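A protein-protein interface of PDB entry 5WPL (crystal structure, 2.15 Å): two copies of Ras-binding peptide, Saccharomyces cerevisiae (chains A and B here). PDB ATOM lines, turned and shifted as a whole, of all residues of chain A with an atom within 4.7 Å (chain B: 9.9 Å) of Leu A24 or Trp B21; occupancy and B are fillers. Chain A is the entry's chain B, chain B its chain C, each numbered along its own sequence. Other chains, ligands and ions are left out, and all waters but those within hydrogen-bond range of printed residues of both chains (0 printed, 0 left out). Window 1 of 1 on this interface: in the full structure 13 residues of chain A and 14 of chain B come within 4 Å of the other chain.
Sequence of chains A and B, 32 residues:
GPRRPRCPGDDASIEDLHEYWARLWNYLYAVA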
ATOM      1  N   PRO A   5     -10.023  12.306   8.245  1.00  0.00           N
ATOM      2  CA  PRO A   5      -9.580  11.077   7.552  1.00  0.00           C
ATOM      3  C   PRO A   5      -9.897  11.081   6.068  1.00  0.00           C
ATOM      4  O   PRO A   5     -10.977  11.523   5.660  1.00  0.00           O
ATOM      5  CB  PRO A   5     -10.364   9.971   8.251  1.00  0.00           C
ATOM      6  CG  PRO A   5     -11.627  10.645   8.648  1.00  0.00           C
ATOM      7  CD  PRO A   5     -11.266  12.063   9.003  1.00  0.00           C
ATOM      8  N   TYR A  20     -12.163   3.171   8.322  1.00  0.00           N
ATOM      9  CA  TYR A  20     -12.510   4.547   8.033  1.00  0.00           C
ATOM     10  C   TYR A  20     -13.597   5.081   8.999  1.00  0.00           C
ATOM     11  O   TYR A  20     -13.434   6.171   9.543  1.00  0.00           O
ATOM     12  CB  TYR A  20     -12.999   4.724   6.585  1.00  0.00           C
ATOM     13  CG  TYR A  20     -13.609   6.089   6.397  1.00  0.00           C
ATOM     14  CD1 TYR A  20     -12.810   7.171   6.130  1.00  0.00           C
ATOM     15  CD2 TYR A  20     -14.969   6.303   6.586  1.00  0.00           C
ATOM     16  CE1 TYR A  20     -13.338   8.445   6.007  1.00  0.00           C
ATOM     17  CE2 TYR A  20     -15.516   7.567   6.486  1.00  0.00           C
ATOM     18  CZ  TYR A  20     -14.682   8.647   6.180  1.00  0.00           C
ATOM     19  OH  TYR A  20     -15.169   9.948   6.045  1.00  0.00           O
ATOM     20  N   TRP A  21     -14.707   4.349   9.149  1.00  0.00           N
ATOM     21  CA  TRP A  21     -15.819   4.749  10.029  1.00  0.00           C
ATOM     22  C   TRP A  21     -15.365   5.050  11.454  1.00  0.00           C
ATOM     23  O   TRP A  21     -15.848   6.001  12.058  1.00  0.00           O
ATOM     24  CB  TRP A  21     -16.914   3.670  10.118  1.00  0.00           C
ATOM     25  CG  TRP A  21     -18.154   4.168  10.825  1.00  0.00           C
ATOM     26  CD1 TRP A  21     -19.172   4.862  10.276  1.00  0.00           C
ATOM     27  CD2 TRP A  21     -18.473   4.016  12.215  1.00  0.00           C
ATOM     28  NE1 TRP A  21     -20.112   5.164  11.230  1.00  0.00           N
ATOM     29  CE2 TRP A  21     -19.697   4.669  12.436  1.00  0.00           C
ATOM     30  CE3 TRP A  21     -17.809   3.427  13.309  1.00  0.00           C
ATOM     31  CZ2 TRP A  21     -20.303   4.726  13.687  1.00  0.00           C
ATOM     32  CZ3 TRP A  21     -18.393   3.494  14.553  1.00  0.00           C
ATOM     33  CH2 TRP A  21     -19.643   4.148  14.733  1.00  0.00           C
ATOM     34  N   ALA A  22     -14.477   4.211  12.002  1.00  0.00           N
ATOM     35  CA  ALA A  22     -14.065   4.350  13.395  1.00  0.00           C
ATOM     36  C   ALA A  22     -13.253   5.631  13.552  1.00  0.00           C
ATOM     37  O   ALA A  22     -13.351   6.322  14.542  1.00  0.00           O
ATOM     38  CB  ALA A  22     -13.267   3.126  13.851  1.00  0.00           C
ATOM     39  N   ARG A  23     -12.416   5.904  12.558  1.00  0.00           N
ATOM     40  CA  ARG A  23     -11.724   7.185  12.415  1.00  0.00           C
ATOM     41  C   ARG A  23     -12.679   8.372  12.295  1.00  0.00           C
ATOM     42  O   ARG A  23     -12.466   9.371  12.936  1.00  0.00           O
ATOM     43  CB  ARG A  23     -10.811   7.176  11.183  1.00  0.00           C
ATOM     44  CG  ARG A  23      -9.627   6.266  11.323  1.00  0.00           C
ATOM     45  CD  ARG A  23      -8.634   6.479  10.213  1.00  0.00           C
ATOM     46  NE  ARG A  23      -7.581   5.470  10.318  1.00  0.00           N
ATOM     47  CZ  ARG A  23      -7.381   4.449   9.471  1.00  0.00           C
ATOM     48  NH1 ARG A  23      -8.142   4.245   8.376  1.00  0.00           N
ATOM     49  NH2 ARG A  23      -6.370   3.625   9.732  1.00  0.00           N
ATOM     50  N   LEU A  24     -13.716   8.272  11.466  1.00  0.00           N
ATOM     51  CA  LEU A  24     -14.636   9.394  11.285  1.00  0.00           C
ATOM     52  C   LEU A  24     -15.355   9.720  12.567  1.00  0.00           C
ATOM     53  O   LEU A  24     -15.546  10.886  12.894  1.00  0.00           O
ATOM     54  CB  LEU A  24     -15.651   9.124  10.168  1.00  0.00           C
ATOM     55  CG  LEU A  24     -16.570  10.287   9.771  1.00  0.00           C
ATOM     56  CD1 LEU A  24     -15.776  11.543   9.471  1.00  0.00           C
ATOM     57  CD2 LEU A  24     -17.435   9.888   8.573  1.00  0.00           C
ATOM     58  N   TRP A  25     -15.793   8.677  13.254  1.00  0.00           N
ATOM     59  CA  TRP A  25     -16.369   8.752  14.596  1.00  0.00           C
ATOM     60  C   TRP A  25     -15.539   9.620  15.546  1.00  0.00           C
ATOM     61  O   TRP A  25     -16.082  10.520  16.184  1.00  0.00           O
ATOM     62  CB  TRP A  25     -16.461   7.321  15.164  1.00  0.00           C
ATOM     63  CG  TRP A  25     -17.378   7.043  16.278  1.00  0.00           C
ATOM     64  CD1 TRP A  25     -18.502   7.714  16.610  1.00  0.00           C
ATOM     65  CD2 TRP A  25     -17.283   5.941  17.176  1.00  0.00           C
ATOM     66  NE1 TRP A  25     -19.101   7.123  17.686  1.00  0.00           N
ATOM     67  CE2 TRP A  25     -18.372   6.027  18.055  1.00  0.00           C
ATOM     68  CE3 TRP A  25     -16.365   4.898  17.331  1.00  0.00           C
ATOM     69  CZ2 TRP A  25     -18.608   5.092  19.047  1.00  0.00           C
ATOM     70  CZ3 TRP A  25     -16.562   3.980  18.352  1.00  0.00           C
ATOM     71  CH2 TRP A  25     -17.678   4.071  19.193  1.00  0.00           C
ATOM     72  N   ASN A  26     -14.245   9.346  15.642  1.00  0.00           N
ATOM     73  CA  ASN A  26     -13.343  10.121  16.509  1.00  0.00           C
ATOM     74  C   ASN A  26     -13.108  11.548  16.067  1.00  0.00           C
ATOM     75  O   ASN A  26     -13.053  12.458  16.906  1.00  0.00           O
ATOM     76  CB  ASN A  26     -11.994   9.430  16.704  1.00  0.00           C
ATOM     77  CG  ASN A  26     -12.100   8.267  17.671  1.00  0.00           C
ATOM     78  OD1 ASN A  26     -11.921   8.437  18.883  1.00  0.00           O
ATOM     79  ND2 ASN A  26     -12.486   7.114  17.165  1.00  0.00           N
ATOM     80  N   TYR A  27     -12.941  11.726  14.761  1.00  0.00           N
ATOM     81  CA  TYR A  27     -12.834  13.027  14.160  1.00  0.00           C
ATOM     82  C   TYR A  27     -14.041  13.969  14.425  1.00  0.00           C
ATOM     83  O   TYR A  27     -13.853  15.100  14.905  1.00  0.00           O
ATOM     84  CB  TYR A  27     -12.609  12.883  12.647  1.00  0.00           C
ATOM     85  CG  TYR A  27     -12.544  14.219  11.969  1.00  0.00           C
ATOM     86  CD1 TYR A  27     -11.410  14.987  12.056  1.00  0.00           C
ATOM     87  CD2 TYR A  27     -13.646  14.736  11.299  1.00  0.00           C
ATOM     88  CE1 TYR A  27     -11.339  16.223  11.440  1.00  0.00           C
ATOM     89  CE2 TYR A  27     -13.595  15.980  10.692  1.00  0.00           C
ATOM     90  CZ  TYR A  27     -12.429  16.706  10.775  1.00  0.00           C
ATOM     91  OH  TYR A  27     -12.372  17.928  10.209  1.00  0.00           O
ATOM     92  N   LEU A  28     -15.244  13.501  14.110  1.00  0.00           N
ATOM     93  CA  LEU A  28     -16.456  14.296  14.317  1.00  0.00           C
ATOM     94  C   LEU A  28     -16.729  14.639  15.798  1.00  0.00           C
ATOM     95  O   LEU A  28     -17.226  15.726  16.104  1.00  0.00           O
ATOM     96  CB  LEU A  28     -17.665  13.612  13.728  1.00  0.00           C
ATOM     97  CG  LEU A  28     -17.677  13.413  12.206  1.00  0.00           C
ATOM     98  CD1 LEU A  28     -18.799  12.470  11.805  1.00  0.00           C
ATOM     99  CD2 LEU A  28     -17.812  14.731  11.473  1.00  0.00           C
ATOM    100  N   PRO B   5     -23.019   4.436   0.651  1.00  0.00           N
ATOM    101  CA  PRO B   5     -22.977   5.901   0.522  1.00  0.00           C
ATOM    102  C   PRO B   5     -21.627   6.391  -0.025  1.00  0.00           C
ATOM    103  O   PRO B   5     -20.638   5.657  -0.005  1.00  0.00           O
ATOM    104  CB  PRO B   5     -23.264   6.388   1.954  1.00  0.00           C
ATOM    105  CG  PRO B   5     -22.785   5.262   2.815  1.00  0.00           C
ATOM    106  CD  PRO B   5     -23.171   4.026   2.062  1.00  0.00           C
ATOM    107  N   ARG B   6     -21.605   7.608  -0.545  1.00  0.00           N
ATOM    108  CA  ARG B   6     -20.424   8.128  -1.207  1.00  0.00           C
ATOM    109  C   ARG B   6     -19.804   9.100  -0.230  1.00  0.00           C
ATOM    110  O   ARG B   6     -20.494   9.908   0.391  1.00  0.00           O
ATOM    111  CB  ARG B   6     -20.764   8.793  -2.559  1.00  0.00           C
ATOM    112  CG  ARG B   6     -21.955   8.180  -3.319  1.00  0.00           C
ATOM    113  CD  ARG B   6     -23.262   8.967  -3.085  1.00  0.00           C
ATOM    114  NE  ARG B   6     -24.470   8.146  -2.810  1.00  0.00           N
ATOM    115  CZ  ARG B   6     -25.176   8.100  -1.659  1.00  0.00           C
ATOM    116  NH1 ARG B   6     -26.251   7.304  -1.600  1.00  0.00           N
ATOM    117  NH2 ARG B   6     -24.849   8.820  -0.564  1.00  0.00           N
ATOM    118  N   CYS B   7     -18.506   8.991  -0.053  1.00  0.00           N
ATOM    119  CA  CYS B   7     -17.782   9.851   0.863  1.00  0.00           C
ATOM    120  C   CYS B   7     -17.749  11.218   0.224  1.00  0.00           C
ATOM    121  O   CYS B   7     -17.514  11.292  -0.972  1.00  0.00           O
ATOM    122  CB  CYS B   7     -16.364   9.335   1.007  1.00  0.00           C
ATOM    123  SG  CYS B   7     -15.396  10.205   2.251  1.00  0.00           S
ATOM    124  N   PRO B   8     -18.011  12.299   0.992  1.00  0.00           N
ATOM    125  CA  PRO B   8     -18.043  13.601   0.318  1.00  0.00           C
ATOM    126  C   PRO B   8     -16.644  14.208   0.151  1.00  0.00           C
ATOM    127  O   PRO B   8     -15.696  13.826   0.852  1.00  0.00           O
ATOM    128  CB  PRO B   8     -18.939  14.457   1.236  1.00  0.00           C
ATOM    129  CG  PRO B   8     -18.798  13.863   2.579  1.00  0.00           C
ATOM    130  CD  PRO B   8     -18.491  12.397   2.388  1.00  0.00           C
ATOM    131  N   SER B  13     -19.182  20.140   4.476  1.00  0.00           N
ATOM    132  CA  SER B  13     -19.358  20.551   5.862  1.00  0.00           C
ATOM    133  C   SER B  13     -19.165  19.374   6.823  1.00  0.00           C
ATOM    134  O   SER B  13     -19.184  18.195   6.416  1.00  0.00           O
ATOM    135  CB  SER B  13     -20.732  21.202   6.061  1.00  0.00           C
ATOM    136  OG  SER B  13     -21.808  20.303   5.947  1.00  0.00           O
ATOM    137  N   ILE B  14     -19.002  19.711   8.099  1.00  0.00           N
ATOM    138  CA  ILE B  14     -19.006  18.715   9.169  1.00  0.00           C
ATOM    139  C   ILE B  14     -20.366  18.047   9.249  1.00  0.00           C
ATOM    140  O   ILE B  14     -20.441  16.822   9.448  1.00  0.00           O
ATOM    141  CB  ILE B  14     -18.472  19.319  10.476  1.00  0.00           C
ATOM    142  CG1 ILE B  14     -16.932  19.333  10.394  1.00  0.00           C
ATOM    143  CG2 ILE B  14     -18.927  18.530  11.698  1.00  0.00           C
ATOM    144  CD1 ILE B  14     -16.269  20.540  11.015  1.00  0.00           C
ATOM    145  N   GLU B  15     -21.442  18.794   9.021  1.00  0.00           N
ATOM    146  CA  GLU B  15     -22.754  18.142   8.936  1.00  0.00           C
ATOM    147  C   GLU B  15     -22.863  17.140   7.750  1.00  0.00           C
ATOM    148  O   GLU B  15     -23.637  16.200   7.832  1.00  0.00           O
ATOM    149  CB  GLU B  15     -23.881  19.173   8.810  1.00  0.00           C
ATOM    150  CG  GLU B  15     -25.260  18.551   8.884  1.00  0.00           C
ATOM    151  CD  GLU B  15     -26.415  19.510   8.639  1.00  0.00           C
ATOM    152  OE1 GLU B  15     -26.291  20.457   7.799  1.00  0.00           O
ATOM    153  OE2 GLU B  15     -27.485  19.243   9.232  1.00  0.00           O
ATOM    154  N   ASP B  16     -22.200  17.430   6.619  1.00  0.00           N
ATOM    155  CA  ASP B  16     -22.159  16.506   5.477  1.00  0.00           C
ATOM    156  C   ASP B  16     -21.327  15.273   5.891  1.00  0.00           C
ATOM    157  O   ASP B  16     -21.702  14.172   5.565  1.00  0.00           O
ATOM    158  CB  ASP B  16     -21.530  17.127   4.226  1.00  0.00           C
ATOM    159  CG  ASP B  16     -22.357  18.257   3.600  1.00  0.00           C
ATOM    160  OD1 ASP B  16     -23.605  18.334   3.699  1.00  0.00           O
ATOM    161  OD2 ASP B  16     -21.722  19.102   2.968  1.00  0.00           O
ATOM    162  N   LEU B  17     -20.213  15.456   6.600  1.00  0.00           N
ATOM    163  CA  LEU B  17     -19.473  14.295   7.171  1.00  0.00           C
ATOM    164  C   LEU B  17     -20.287  13.499   8.169  1.00  0.00           C
ATOM    165  O   LEU B  17     -20.319  12.275   8.116  1.00  0.00           O
ATOM    166  CB  LEU B  17     -18.156  14.708   7.789  1.00  0.00           C
ATOM    167  CG  LEU B  17     -17.143  15.156   6.746  1.00  0.00           C
ATOM    168  CD1 LEU B  17     -15.939  15.745   7.442  1.00  0.00           C
ATOM    169  CD2 LEU B  17     -16.704  14.007   5.831  1.00  0.00           C
ATOM    170  N   HIS B  18     -20.987  14.201   9.040  1.00  0.00           N
ATOM    171  CA  HIS B  18     -21.965  13.571   9.914  1.00  0.00           C
ATOM    172  C   HIS B  18     -22.971  12.690   9.204  1.00  0.00           C
ATOM    173  O   HIS B  18     -23.248  11.552   9.637  1.00  0.00           O
ATOM    174  CB  HIS B  18     -22.726  14.624  10.723  1.00  0.00           C
ATOM    175  CG  HIS B  18     -23.587  14.038  11.779  1.00  0.00           C
ATOM    176  ND1 HIS B  18     -23.091  13.653  13.002  1.00  0.00           N
ATOM    177  CD2 HIS B  18     -24.901  13.732  11.789  1.00  0.00           C
ATOM    178  CE1 HIS B  18     -24.071  13.167  13.735  1.00  0.00           C
ATOM    179  NE2 HIS B  18     -25.175  13.186  13.015  1.00  0.00           N
ATOM    180  N   GLU B  19     -23.541  13.227   8.126  1.00  0.00           N
ATOM    181  CA  GLU B  19     -24.515  12.498   7.334  1.00  0.00           C
ATOM    182  C   GLU B  19     -23.945  11.206   6.786  1.00  0.00           C
ATOM    183  O   GLU B  19     -24.595  10.186   6.839  1.00  0.00           O
ATOM    184  CB  GLU B  19     -25.021  13.359   6.179  1.00  0.00           C
ATOM    185  CG  GLU B  19     -26.058  14.423   6.584  1.00  0.00           C
ATOM    186  CD  GLU B  19     -26.060  15.626   5.650  1.00  0.00           C
ATOM    187  OE1 GLU B  19     -26.687  16.654   6.012  1.00  0.00           O
ATOM    188  OE2 GLU B  19     -25.422  15.562   4.563  1.00  0.00           O
ATOM    189  N   TYR B  20     -22.744  11.278   6.237  1.00  0.00           N
ATOM    190  CA  TYR B  20     -22.018  10.107   5.736  1.00  0.00           C
ATOM    191  C   TYR B  20     -21.764   9.105   6.880  1.00  0.00           C
ATOM    192  O   TYR B  20     -22.072   7.929   6.777  1.00  0.00           O
ATOM    193  CB  TYR B  20     -20.716  10.576   5.101  1.00  0.00           C
ATOM    194  CG  TYR B  20     -19.819   9.491   4.518  1.00  0.00           C
ATOM    195  CD1 TYR B  20     -20.325   8.524   3.658  1.00  0.00           C
ATOM    196  CD2 TYR B  20     -18.466   9.479   4.779  1.00  0.00           C
ATOM    197  CE1 TYR B  20     -19.514   7.539   3.121  1.00  0.00           C
ATOM    198  CE2 TYR B  20     -17.641   8.499   4.232  1.00  0.00           C
ATOM    199  CZ  TYR B  20     -18.167   7.511   3.410  1.00  0.00           C
ATOM    200  OH  TYR B  20     -17.311   6.555   2.828  1.00  0.00           O
ATOM    201  N   TRP B  21     -21.254   9.615   7.988  1.00  0.00           N
ATOM    202  CA  TRP B  21     -21.064   8.818   9.210  1.00  0.00           C
ATOM    203  C   TRP B  21     -22.276   7.967   9.555  1.00  0.00           C
ATOM    204  O   TRP B  21     -22.141   6.749   9.716  1.00  0.00           O
ATOM    205  CB  TRP B  21     -20.733   9.745  10.378  1.00  0.00           C
ATOM    206  CG  TRP B  21     -20.577   9.036  11.651  1.00  0.00           C
ATOM    207  CD1 TRP B  21     -19.458   8.404  12.089  1.00  0.00           C
ATOM    208  CD2 TRP B  21     -21.554   8.894  12.674  1.00  0.00           C
ATOM    209  NE1 TRP B  21     -19.685   7.863  13.321  1.00  0.00           N
ATOM    210  CE2 TRP B  21     -20.966   8.149  13.706  1.00  0.00           C
ATOM    211  CE3 TRP B  21     -22.879   9.305  12.811  1.00  0.00           C
ATOM    212  CZ2 TRP B  21     -21.667   7.781  14.863  1.00  0.00           C
ATOM    213  CZ3 TRP B  21     -23.576   8.971  13.972  1.00  0.00           C
ATOM    214  CH2 TRP B  21     -22.967   8.215  14.980  1.00  0.00           C
ATOM    215  N   ALA B  22     -23.451   8.605   9.613  1.00  0.00           N
ATOM    216  CA  ALA B  22     -24.729   7.922   9.863  1.00  0.00           C
ATOM    217  C   ALA B  22     -25.134   6.947   8.753  1.00  0.00           C
ATOM    218  O   ALA B  22     -25.566   5.849   9.031  1.00  0.00           O
ATOM    219  CB  ALA B  22     -25.875   8.943  10.071  1.00  0.00           C
ATOM    220  N   ARG B  23     -25.055   7.377   7.503  1.00  0.00           N
ATOM    221  CA  ARG B  23     -25.366   6.504   6.378  1.00  0.00           C
ATOM    222  C   ARG B  23     -24.426   5.291   6.326  1.00  0.00           C
ATOM    223  O   ARG B  23     -24.865   4.192   6.026  1.00  0.00           O
ATOM    224  CB  ARG B  23     -25.292   7.258   5.037  1.00  0.00           C
ATOM    225  CG  ARG B  23     -26.618   7.838   4.550  1.00  0.00           C
ATOM    226  CD  ARG B  23     -26.808   9.288   4.952  1.00  0.00           C
ATOM    227  NE  ARG B  23     -28.093   9.867   4.538  1.00  0.00           N
ATOM    228  CZ  ARG B  23     -28.420  10.231   3.295  1.00  0.00           C
ATOM    229  NH1 ARG B  23     -29.619  10.767   3.059  1.00  0.00           N
ATOM    230  NH2 ARG B  23     -27.564  10.067   2.285  1.00  0.00           N
ATOM    231  N   LEU B  24     -23.145   5.515   6.617  1.00  0.00           N
ATOM    232  CA  LEU B  24     -22.158   4.458   6.547  1.00  0.00           C
ATOM    233  C   LEU B  24     -22.374   3.445   7.648  1.00  0.00           C
ATOM    234  O   LEU B  24     -22.260   2.252   7.398  1.00  0.00           O
ATOM    235  CB  LEU B  24     -20.734   5.026   6.544  1.00  0.00           C
ATOM    236  CG  LEU B  24     -19.569   4.065   6.374  1.00  0.00           C
ATOM    237  CD1 LEU B  24     -19.643   3.268   5.084  1.00  0.00           C
ATOM    238  CD2 LEU B  24     -18.260   4.825   6.398  1.00  0.00           C
ATOM    239  N   TRP B  25     -22.747   3.895   8.846  1.00  0.00           N
ATOM    240  CA  TRP B  25     -23.202   2.980   9.916  1.00  0.00           C
ATOM    241  C   TRP B  25     -24.411   2.140   9.483  1.00  0.00           C
ATOM    242  O   TRP B  25     -24.447   0.941   9.775  1.00  0.00           O
ATOM    243  CB  TRP B  25     -23.532   3.733  11.219  1.00  0.00           C
ATOM    244  CG  TRP B  25     -23.759   2.823  12.395  1.00  0.00           C
ATOM    245  CD1 TRP B  25     -22.830   2.416  13.299  1.00  0.00           C
ATOM    246  CD2 TRP B  25     -24.982   2.186  12.764  1.00  0.00           C
ATOM    247  NE1 TRP B  25     -23.394   1.564  14.209  1.00  0.00           N
ATOM    248  CE2 TRP B  25     -24.717   1.404  13.904  1.00  0.00           C
ATOM    249  CE3 TRP B  25     -26.279   2.181  12.227  1.00  0.00           C
ATOM    250  CZ2 TRP B  25     -25.699   0.628  14.527  1.00  0.00           C
ATOM    251  CZ3 TRP B  25     -27.268   1.405  12.853  1.00  0.00           C
ATOM    252  CH2 TRP B  25     -26.968   0.640  13.985  1.00  0.00           C
ATOM    253  N   ASN B  26     -25.409   2.765   8.838  1.00  0.00           N
ATOM    254  CA  ASN B  26     -26.593   2.042   8.380  1.00  0.00           C
ATOM    255  C   ASN B  26     -26.224   0.981   7.343  1.00  0.00           C
ATOM    256  O   ASN B  26     -26.676  -0.146   7.428  1.00  0.00           O
ATOM    257  CB  ASN B  26     -27.671   2.968   7.792  1.00  0.00           C
ATOM    258  CG  ASN B  26     -28.313   3.872   8.845  1.00  0.00           C
ATOM    259  OD1 ASN B  26     -28.385   3.516  10.024  1.00  0.00           O
ATOM    260  ND2 ASN B  26     -28.763   5.074   8.423  1.00  0.00           N
ATOM    261  N   TYR B  27     -25.433   1.375   6.362  1.00  0.00           N
ATOM    262  CA  TYR B  27     -24.969   0.463   5.338  1.00  0.00           C
ATOM    263  C   TYR B  27     -24.145  -0.718   5.948  1.00  0.00           C
ATOM    264  O   TYR B  27     -24.458  -1.869   5.697  1.00  0.00           O
ATOM    265  CB  TYR B  27     -24.154   1.232   4.303  1.00  0.00           C
ATOM    266  CG  TYR B  27     -23.484   0.349   3.273  1.00  0.00           C
ATOM    267  CD1 TYR B  27     -24.208  -0.215   2.211  1.00  0.00           C
ATOM    268  CD2 TYR B  27     -22.134   0.081   3.362  1.00  0.00           C
ATOM    269  CE1 TYR B  27     -23.570  -1.020   1.263  1.00  0.00           C
ATOM    270  CE2 TYR B  27     -21.502  -0.722   2.440  1.00  0.00           C
ATOM    271  CZ  TYR B  27     -22.202  -1.271   1.405  1.00  0.00           C
ATOM    272  OH  TYR B  27     -21.490  -2.062   0.539  1.00  0.00           O
ATOM    273  N   LEU B  28     -23.137  -0.412   6.772  1.00  0.00           N
ATOM    274  CA  LEU B  28     -22.346  -1.442   7.433  1.00  0.00           C
ATOM    275  C   LEU B  28     -23.151  -2.366   8.347  1.00  0.00           C
ATOM    276  O   LEU B  28     -22.799  -3.520   8.496  1.00  0.00           O
ATOM    277  CB  LEU B  28     -21.202  -0.819   8.207  1.00  0.00           C
ATOM    278  CG  LEU B  28     -20.126  -0.160   7.370  1.00  0.00           C
ATOM    279  CD1 LEU B  28     -19.154   0.577   8.261  1.00  0.00           C
ATOM    280  CD2 LEU B  28     -19.390  -1.202   6.526  1.00  0.00           C
ATOM    281  N   TYR B  29     -24.233  -1.876   8.935  1.00  0.00           N
ATOM    282  CA  TYR B  29     -25.122  -2.702   9.754  1.00  0.00           C
ATOM    283  C   TYR B  29     -26.002  -3.592   8.873  1.00  0.00           C
ATOM    284  O   TYR B  29     -26.287  -4.748   9.225  1.00  0.00           O
ATOM    285  CB  TYR B  29     -26.027  -1.814  10.626  1.00  0.00           C
ATOM    286  CG  TYR B  29     -27.030  -2.593  11.475  1.00  0.00           C
ATOM    287  CD1 TYR B  29     -26.682  -3.079  12.745  1.00  0.00           C
ATOM    288  CD2 TYR B  29     -28.319  -2.855  10.985  1.00  0.00           C
ATOM    289  CE1 TYR B  29     -27.594  -3.780  13.515  1.00  0.00           C
ATOM    290  CE2 TYR B  29     -29.231  -3.578  11.727  1.00  0.00           C
ATOM    291  CZ  TYR B  29     -28.866  -4.037  13.000  1.00  0.00           C
ATOM    292  OH  TYR B  29     -29.800  -4.755  13.738  1.00  0.00           O
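Among the printed residues, pairs that only touch across the chains: Tyr A20 with Cys B7 (3.8 Å), Tyr A20 with Tyr B20 (3.2 Å), Tyr A20 with Leu B24 (3.6 Å), Trp A21 with Leu B24 (3.98 Å), Trp A21 with Trp B25 (3.4 Å), Leu A24 with Leu B17 (3.8 Å), Leu A24 with Tyr B20 (3.95 Å), Leu A24 with Trp B21 (3.8 Å), Trp A25 with Trp B21 (3.5 Å), Leu A28 with Ile B14 (3.9 Å), Leu A28 with Leu B17 (3.7 Å), Leu A28 with His B18 (3.8 Å) and Leu A28 with Trp B21 (3.6 Å).
Trp A21 touches its own counterpart, Trp B21. Trp A21 touches Leu B24, and with the chains exchanged Leu A24 touches Trp B21. Trp A21 touches Trp B25, and with the chains exchanged Trp A25 touches Trp B21. Leu A28 touches Trp B21, but with the chains exchanged Trp A21 does not touch Leu B28 (4.2 Å).
The backbone carbonyl oxygen (O) of Trp B21 sits at hydrogen-bond distance from the indole nitrogen (NE1) of Trp A21, at 3.0 Å.
Of the 10 printed residues of chain A, 5 touch a printed residue of chain B. Hydrophobic or aromatic side chains of chain A that line the printed part of chain B: Tyr A20, Trp A21, Leu A24, Trp A25 and Leu A28.
Leu A24 touches three residues of chain B. Of the printed residues of chain A, Trp B21 touches Trp A21, Leu A24, Trp A25 and Leu A28. No residue of chain B comes within 4 Å of Ala A22. Of the printed residues of chain A, Leu B17 touches Leu A24 (3.8 Å) and Leu A28 (3.7 Å). Of the printed residues of chain B, Tyr A20 touches Cys B7 (3.8 Å), Tyr B20 (3.2 Å) and Leu B24 (3.6 Å). Printed residues of chain B within 4 Å of Trp A25: Trp B21 (3.5 Å). Printed residues of chain A within 4 Å of Tyr B20: Tyr A20 (3.2 Å) and Leu A24 (3.95 Å). Asn A26 touches none of the printed residues of chain B.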
